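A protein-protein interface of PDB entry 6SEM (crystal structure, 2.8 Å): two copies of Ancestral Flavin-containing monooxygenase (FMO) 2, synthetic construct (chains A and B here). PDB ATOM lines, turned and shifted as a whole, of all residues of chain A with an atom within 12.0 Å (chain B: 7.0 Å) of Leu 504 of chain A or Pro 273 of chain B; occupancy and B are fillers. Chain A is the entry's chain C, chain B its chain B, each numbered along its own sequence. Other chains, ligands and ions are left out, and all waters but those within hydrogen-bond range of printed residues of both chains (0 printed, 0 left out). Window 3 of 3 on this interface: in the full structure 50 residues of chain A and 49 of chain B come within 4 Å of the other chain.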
ATOM      1  N   LEU A 499      24.710  -9.538 -23.803  1.00  0.00           N
ATOM      2  CA  LEU A 499      23.635  -9.098 -22.895  1.00  0.00           C
ATOM      3  C   LEU A 499      24.159  -8.962 -21.462  1.00  0.00           C
ATOM      4  O   LEU A 499      24.137  -7.874 -20.903  1.00  0.00           O
ATOM      5  CB  LEU A 499      22.499 -10.125 -22.890  1.00  0.00           C
ATOM      6  CG  LEU A 499      21.525 -10.062 -24.051  1.00  0.00           C
ATOM      7  CD1 LEU A 499      20.319 -10.935 -23.745  1.00  0.00           C
ATOM      8  CD2 LEU A 499      21.123  -8.624 -24.345  1.00  0.00           C
ATOM      9  N   LYS A 500      24.527 -10.111 -20.882  1.00  0.00           N
ATOM     10  CA  LYS A 500      24.930 -10.227 -19.499  1.00  0.00           C
ATOM     11  C   LYS A 500      26.289  -9.561 -19.363  1.00  0.00           C
ATOM     12  O   LYS A 500      27.302 -10.203 -19.484  1.00  0.00           O
ATOM     13  CB  LYS A 500      24.961 -11.688 -19.060  1.00  0.00           C
ATOM     14  CG  LYS A 500      24.797 -11.900 -17.568  1.00  0.00           C
ATOM     15  CD  LYS A 500      24.651 -13.379 -17.245  1.00  0.00           C
ATOM     16  CE  LYS A 500      24.087 -13.656 -15.872  1.00  0.00           C
ATOM     17  NZ  LYS A 500      24.765 -14.798 -15.196  1.00  0.00           N
ATOM     18  N   THR A 501      26.243  -8.250 -19.150  1.00  0.00           N
ATOM     19  CA  THR A 501      27.353  -7.346 -19.343  1.00  0.00           C
ATOM     20  C   THR A 501      27.736  -6.725 -17.985  1.00  0.00           C
ATOM     21  O   THR A 501      28.645  -5.890 -17.886  1.00  0.00           O
ATOM     22  CB  THR A 501      26.943  -6.399 -20.478  1.00  0.00           C
ATOM     23  OG1 THR A 501      28.042  -5.587 -20.881  1.00  0.00           O
ATOM     24  CG2 THR A 501      25.796  -5.485 -20.110  1.00  0.00           C
ATOM     25  N   ARG A 502      27.039  -7.206 -16.942  1.00  0.00           N
ATOM     26  CA  ARG A 502      27.207  -6.852 -15.549  1.00  0.00           C
ATOM     27  C   ARG A 502      26.691  -8.027 -14.706  1.00  0.00           C
ATOM     28  O   ARG A 502      25.599  -8.545 -14.960  1.00  0.00           O
ATOM     29  CB  ARG A 502      26.449  -5.560 -15.233  1.00  0.00           C
ATOM     30  CG  ARG A 502      26.815  -4.946 -13.889  1.00  0.00           C
ATOM     31  CD  ARG A 502      25.660  -4.279 -13.180  1.00  0.00           C
ATOM     32  NE  ARG A 502      25.046  -5.165 -12.213  1.00  0.00           N
ATOM     33  CZ  ARG A 502      24.089  -4.802 -11.377  1.00  0.00           C
ATOM     34  NH1 ARG A 502      23.621  -5.665 -10.496  1.00  0.00           N
ATOM     35  NH2 ARG A 502      23.603  -3.578 -11.402  1.00  0.00           N
ATOM     36  N   ALA A 503      27.485  -8.450 -13.714  1.00  0.00           N
ATOM     37  CA  ALA A 503      27.291  -9.719 -13.057  1.00  0.00           C
ATOM     38  C   ALA A 503      27.349  -9.580 -11.528  1.00  0.00           C
ATOM     39  O   ALA A 503      28.136  -8.799 -11.004  1.00  0.00           O
ATOM     40  CB  ALA A 503      28.351 -10.644 -13.572  1.00  0.00           C
ATOM     41  N   LEU A 504      26.512 -10.363 -10.834  1.00  0.00           N
ATOM     42  CA  LEU A 504      26.272 -10.190  -9.415  1.00  0.00           C
ATOM     43  C   LEU A 504      27.299 -10.963  -8.585  1.00  0.00           C
ATOM     44  O   LEU A 504      27.884 -10.378  -7.680  1.00  0.00           O
ATOM     45  CB  LEU A 504      24.840 -10.623  -9.090  1.00  0.00           C
ATOM     46  CG  LEU A 504      24.134  -9.776  -8.031  1.00  0.00           C
ATOM     47  CD1 LEU A 504      24.072  -8.310  -8.440  1.00  0.00           C
ATOM     48  CD2 LEU A 504      22.741 -10.318  -7.737  1.00  0.00           C
ATOM     49  N   LYS A 505      27.501 -12.250  -8.878  1.00  0.00           N
ATOM     50  CA  LYS A 505      28.485 -13.119  -8.145  1.00  0.00           C
ATOM     51  C   LYS A 505      27.904 -13.493  -6.771  1.00  0.00           C
ATOM     52  O   LYS A 505      28.004 -12.733  -5.821  1.00  0.00           O
ATOM     53  CB  LYS A 505      29.873 -12.455  -8.079  1.00  0.00           C
ATOM     54  CG  LYS A 505      30.221 -11.618  -6.838  1.00  0.00           C
ATOM     55  CD  LYS A 505      30.979 -10.305  -7.088  1.00  0.00           C
ATOM     56  CE  LYS A 505      32.478 -10.441  -7.222  1.00  0.00           C
ATOM     57  NZ  LYS A 505      33.061  -9.188  -7.751  1.00  0.00           N
ATOM     58  N   ALA A 506      27.247 -14.655  -6.698  1.00  0.00           N
ATOM     59  CA  ALA A 506      26.425 -15.052  -5.528  1.00  0.00           C
ATOM     60  C   ALA A 506      25.962 -16.508  -5.674  1.00  0.00           C
ATOM     61  O   ALA A 506      26.464 -17.286  -6.499  1.00  0.00           O
ATOM     62  CB  ALA A 506      25.231 -14.131  -5.365  1.00  0.00           C
ATOM     63  N   ARG B 215      26.334  -0.320  -9.627  1.00  0.00           N
ATOM     64  CA  ARG B 215      26.640  -1.467  -8.801  1.00  0.00           C
ATOM     65  C   ARG B 215      25.332  -2.205  -8.548  1.00  0.00           C
ATOM     66  O   ARG B 215      25.229  -3.429  -8.747  1.00  0.00           O
ATOM     67  CB  ARG B 215      27.244  -1.055  -7.464  1.00  0.00           C
ATOM     68  CG  ARG B 215      28.761  -1.106  -7.407  1.00  0.00           C
ATOM     69  CD  ARG B 215      29.332   0.044  -6.586  1.00  0.00           C
ATOM     70  NE  ARG B 215      29.314  -0.212  -5.153  1.00  0.00           N
ATOM     71  CZ  ARG B 215      30.190   0.285  -4.303  1.00  0.00           C
ATOM     72  NH1 ARG B 215      30.122  -0.036  -3.025  1.00  0.00           N
ATOM     73  NH2 ARG B 215      31.156   1.065  -4.748  1.00  0.00           N
ATOM     74  N   HIS B 216      24.334  -1.419  -8.140  1.00  0.00           N
ATOM     75  CA  HIS B 216      23.150  -1.941  -7.506  1.00  0.00           C
ATOM     76  C   HIS B 216      22.186  -2.435  -8.586  1.00  0.00           C
ATOM     77  O   HIS B 216      21.730  -3.568  -8.505  1.00  0.00           O
ATOM     78  CB  HIS B 216      22.560  -0.876  -6.562  1.00  0.00           C
ATOM     79  CG  HIS B 216      23.602  -0.147  -5.779  1.00  0.00           C
ATOM     80  ND1 HIS B 216      24.066  -0.574  -4.533  1.00  0.00           N
ATOM     81  CD2 HIS B 216      24.294   0.971  -6.073  1.00  0.00           C
ATOM     82  CE1 HIS B 216      25.002   0.245  -4.109  1.00  0.00           C
ATOM     83  NE2 HIS B 216      25.151   1.211  -5.028  1.00  0.00           N
ATOM     84  N   GLY B 217      21.910  -1.569  -9.572  1.00  0.00           N
ATOM     85  CA  GLY B 217      21.117  -1.901 -10.734  1.00  0.00           C
ATOM     86  C   GLY B 217      19.674  -2.250 -10.380  1.00  0.00           C
ATOM     87  O   GLY B 217      19.412  -3.209  -9.691  1.00  0.00           O
ATOM     88  N   SER B 218      18.732  -1.485 -10.916  1.00  0.00           N
ATOM     89  CA  SER B 218      17.338  -1.541 -10.524  1.00  0.00           C
ATOM     90  C   SER B 218      16.598  -2.657 -11.266  1.00  0.00           C
ATOM     91  O   SER B 218      17.119  -3.280 -12.173  1.00  0.00           O
ATOM     92  CB  SER B 218      16.667  -0.221 -10.784  1.00  0.00           C
ATOM     93  OG  SER B 218      15.270  -0.312 -10.559  1.00  0.00           O
ATOM     94  N   TRP B 219      15.362  -2.892 -10.819  1.00  0.00           N
ATOM     95  CA  TRP B 219      14.353  -3.526 -11.610  1.00  0.00           C
ATOM     96  C   TRP B 219      13.800  -2.490 -12.599  1.00  0.00           C
ATOM     97  O   TRP B 219      13.504  -1.349 -12.239  1.00  0.00           O
ATOM     98  CB  TRP B 219      13.241  -4.084 -10.718  1.00  0.00           C
ATOM     99  CG  TRP B 219      13.564  -5.366 -10.019  1.00  0.00           C
ATOM    100  CD1 TRP B 219      14.162  -6.479 -10.540  1.00  0.00           C
ATOM    101  CD2 TRP B 219      13.247  -5.686  -8.657  1.00  0.00           C
ATOM    102  NE1 TRP B 219      14.266  -7.463  -9.588  1.00  0.00           N
ATOM    103  CE2 TRP B 219      13.700  -7.006  -8.430  1.00  0.00           C
ATOM    104  CE3 TRP B 219      12.598  -4.999  -7.625  1.00  0.00           C
ATOM    105  CZ2 TRP B 219      13.524  -7.636  -7.197  1.00  0.00           C
ATOM    106  CZ3 TRP B 219      12.442  -5.613  -6.399  1.00  0.00           C
ATOM    107  CH2 TRP B 219      12.901  -6.916  -6.194  1.00  0.00           C
ATOM    108  N   HIS B 266      16.258 -10.426 -15.499  1.00  0.00           N
ATOM    109  CA  HIS B 266      17.106  -9.288 -15.177  1.00  0.00           C
ATOM    110  C   HIS B 266      18.565  -9.726 -14.977  1.00  0.00           C
ATOM    111  O   HIS B 266      19.485  -8.932 -15.142  1.00  0.00           O
ATOM    112  CB  HIS B 266      16.553  -8.550 -13.952  1.00  0.00           C
ATOM    113  CG  HIS B 266      15.317  -7.762 -14.228  1.00  0.00           C
ATOM    114  ND1 HIS B 266      15.192  -6.436 -13.869  1.00  0.00           N
ATOM    115  CD2 HIS B 266      14.160  -8.104 -14.832  1.00  0.00           C
ATOM    116  CE1 HIS B 266      14.001  -6.009 -14.237  1.00  0.00           C
ATOM    117  NE2 HIS B 266      13.349  -7.014 -14.834  1.00  0.00           N
ATOM    118  N   GLU B 267      18.763 -10.984 -14.580  1.00  0.00           N
ATOM    119  CA  GLU B 267      20.099 -11.561 -14.438  1.00  0.00           C
ATOM    120  C   GLU B 267      20.798 -11.516 -15.800  1.00  0.00           C
ATOM    121  O   GLU B 267      21.918 -11.038 -15.909  1.00  0.00           O
ATOM    122  CB  GLU B 267      19.976 -12.981 -13.885  1.00  0.00           C
ATOM    123  CG  GLU B 267      21.268 -13.643 -13.425  1.00  0.00           C
ATOM    124  CD  GLU B 267      21.085 -15.057 -12.868  1.00  0.00           C
ATOM    125  OE1 GLU B 267      20.070 -15.726 -13.204  1.00  0.00           O
ATOM    126  OE2 GLU B 267      21.963 -15.514 -12.092  1.00  0.00           O
ATOM    127  N   GLY B 270      21.455  -8.132 -17.134  1.00  0.00           N
ATOM    128  CA  GLY B 270      22.604  -7.723 -16.350  1.00  0.00           C
ATOM    129  C   GLY B 270      22.288  -6.637 -15.332  1.00  0.00           C
ATOM    130  O   GLY B 270      23.201  -6.020 -14.791  1.00  0.00           O
ATOM    131  N   LEU B 271      21.010  -6.421 -15.014  1.00  0.00           N
ATOM    132  CA  LEU B 271      20.708  -5.398 -14.004  1.00  0.00           C
ATOM    133  C   LEU B 271      19.961  -6.008 -12.816  1.00  0.00           C
ATOM    134  O   LEU B 271      19.240  -5.316 -12.087  1.00  0.00           O
ATOM    135  CB  LEU B 271      19.963  -4.223 -14.654  1.00  0.00           C
ATOM    136  CG  LEU B 271      19.117  -4.536 -15.879  1.00  0.00           C
ATOM    137  CD1 LEU B 271      17.837  -5.255 -15.476  1.00  0.00           C
ATOM    138  CD2 LEU B 271      18.806  -3.257 -16.625  1.00  0.00           C
ATOM    139  N   GLU B 272      20.200  -7.300 -12.585  1.00  0.00           N
ATOM    140  CA  GLU B 272      19.737  -7.935 -11.376  1.00  0.00           C
ATOM    141  C   GLU B 272      20.241  -7.105 -10.211  1.00  0.00           C
ATOM    142  O   GLU B 272      21.427  -6.794 -10.175  1.00  0.00           O
ATOM    143  CB  GLU B 272      20.246  -9.367 -11.253  1.00  0.00           C
ATOM    144  CG  GLU B 272      19.488 -10.180 -10.219  1.00  0.00           C
ATOM    145  CD  GLU B 272      19.990 -11.604 -10.082  1.00  0.00           C
ATOM    146  OE1 GLU B 272      21.220 -11.799 -10.199  1.00  0.00           O
ATOM    147  OE2 GLU B 272      19.149 -12.522  -9.887  1.00  0.00           O
ATOM    148  N   PRO B 273      19.340  -6.671  -9.296  1.00  0.00           N
ATOM    149  CA  PRO B 273      19.729  -6.007  -8.049  1.00  0.00           C
ATOM    150  C   PRO B 273      20.507  -6.869  -7.046  1.00  0.00           C
ATOM    151  O   PRO B 273      20.495  -8.105  -7.136  1.00  0.00           O
ATOM    152  CB  PRO B 273      18.393  -5.642  -7.387  1.00  0.00           C
ATOM    153  CG  PRO B 273      17.386  -5.656  -8.515  1.00  0.00           C
ATOM    154  CD  PRO B 273      17.881  -6.720  -9.466  1.00  0.00           C
ATOM    155  N   GLN B 274      21.160  -6.186  -6.096  1.00  0.00           N
ATOM    156  CA  GLN B 274      21.866  -6.847  -4.989  1.00  0.00           C
ATOM    157  C   GLN B 274      20.835  -7.253  -3.930  1.00  0.00           C
ATOM    158  O   GLN B 274      20.549  -8.440  -3.770  1.00  0.00           O
ATOM    159  CB  GLN B 274      22.953  -5.945  -4.406  1.00  0.00           C
ATOM    160  CG  GLN B 274      24.065  -5.603  -5.397  1.00  0.00           C
ATOM    161  CD  GLN B 274      24.950  -4.482  -4.919  1.00  0.00           C
ATOM    162  OE1 GLN B 274      26.068  -4.311  -5.400  1.00  0.00           O
ATOM    163  NE2 GLN B 274      24.459  -3.717  -3.958  1.00  0.00           N
ATOM    164  N   ASN B 275      20.254  -6.263  -3.244  1.00  0.00           N
ATOM    165  CA  ASN B 275      19.208  -6.511  -2.237  1.00  0.00           C
ATOM    166  C   ASN B 275      17.835  -6.353  -2.898  1.00  0.00           C
ATOM    167  O   ASN B 275      17.351  -5.263  -3.129  1.00  0.00           O
ATOM    168  CB  ASN B 275      19.339  -5.660  -0.965  1.00  0.00           C
ATOM    169  CG  ASN B 275      20.328  -4.521  -1.087  1.00  0.00           C
ATOM    170  OD1 ASN B 275      20.109  -3.620  -1.887  1.00  0.00           O
ATOM    171  ND2 ASN B 275      21.414  -4.561  -0.325  1.00  0.00           N
ATOM    172  N   LYS B 276      17.230  -7.499  -3.203  1.00  0.00           N
ATOM    173  CA  LYS B 276      15.865  -7.572  -3.650  1.00  0.00           C
ATOM    174  C   LYS B 276      14.950  -7.401  -2.433  1.00  0.00           C
ATOM    175  O   LYS B 276      13.738  -7.220  -2.586  1.00  0.00           O
ATOM    176  CB  LYS B 276      15.654  -8.915  -4.356  1.00  0.00           C
ATOM    177  CG  LYS B 276      16.593  -9.155  -5.526  1.00  0.00           C
ATOM    178  CD  LYS B 276      16.895 -10.605  -5.734  1.00  0.00           C
ATOM    179  CE  LYS B 276      17.994 -10.823  -6.755  1.00  0.00           C
ATOM    180  NZ  LYS B 276      17.678 -11.888  -7.742  1.00  0.00           N
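A ring nitrogen (ND1) of His 216 of chain B is in hydrogen-bond range of the side-chain amide nitrogen of Gln 274 of chain B (3.2 Å).
The backbone NH (N) of Glu 272 of chain B is in hydrogen-bond range of the backbone carbonyl oxygen (O) of His 266 of chain B (3.1 Å).
The side-chain carboxylate (OE2) of Glu 272 of chain B is in salt-bridge range of the side-chain amino group (NZ) of Lys 276 of chain B, at 2.7 Å.
No position is printed for both chains.
Of the 8 pairs that touch across the chains among the printed residues, none has its exchanged pair printed and touching as well.
The backbone carbonyl oxygen (O) of Arg 215 of chain B sits at hydrogen-bond distance from the guanidinium group (NH2) of Arg 502 of chain A, at 3.1 Å.
The guanidinium group (NH2) of Arg 502 of chain A lies close to the backbone carbonyl oxygen (O) of His 216 of chain B (3.4 Å).
The guanidinium group (NE) of Arg 502 of chain A sits at hydrogen-bond distance from the backbone carbonyl oxygen (O) of Gly 270 of chain B (3.3 Å).
The backbone carbonyl oxygen (O) of Glu 272 of chain B is in hydrogen-bond range of the guanidinium group (NH1) of Arg 502 of chain A (2.5 Å).
N of Gly 217 of chain B lies close to NH2 of Arg 502 of chain A (3.2 Å).
O of Glu 267 of chain B touches CE of Lys 500 of chain A (3.4 Å).
OE1 of Glu 272 of chain B touches CD2 of Leu 504 of chain A (3.3 Å).
Leu 504 of chain A touches Pro 273 of chain B.
Of the printed residues of chain B, Arg 502 of chain A touches Arg 215 (3.1 Å), His 216 (3.4 Å), Gly 217 (3.1 Å), Gly 270 (3.3 Å) and Glu 272 (2.5 Å).
Leu 504 of chain A touches two residues of chain B.
Lys 505 of chain A touches none of the printed residues of chain B.
Of the printed residues of chain A, His 216 of chain B touches Arg 502 (3.4 Å).
No residue of chain A comes within 4 Å of Ser 218 of chain B.
No residue of chain A comes within 4 Å of Trp 219 of chain B.
No residue of chain A comes within 4 Å of His 266 of chain B.
Printed residues of chain A within 4 Å of Gly 270 of chain B: Arg 502 (3.3 Å).
No residue of chain A comes within 4 Å of Gln 274 of chain B.
Asn 275 of chain B touches none of the printed residues of chain A.
No residue of chain A comes within 4 Å of Lys 276 of chain B.
The nearest residue of chain A that does not touch Pro 273 of chain B is Arg 502 of chain A (4.6 Å).
Hydrophobic or aromatic side chains of chain A that line the printed part of chain B: Leu 504.
Among the printed residues, no Asp or Glu carboxylate lies within 4 Å of a Lys or Arg side-chain nitrogen of the other chain.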
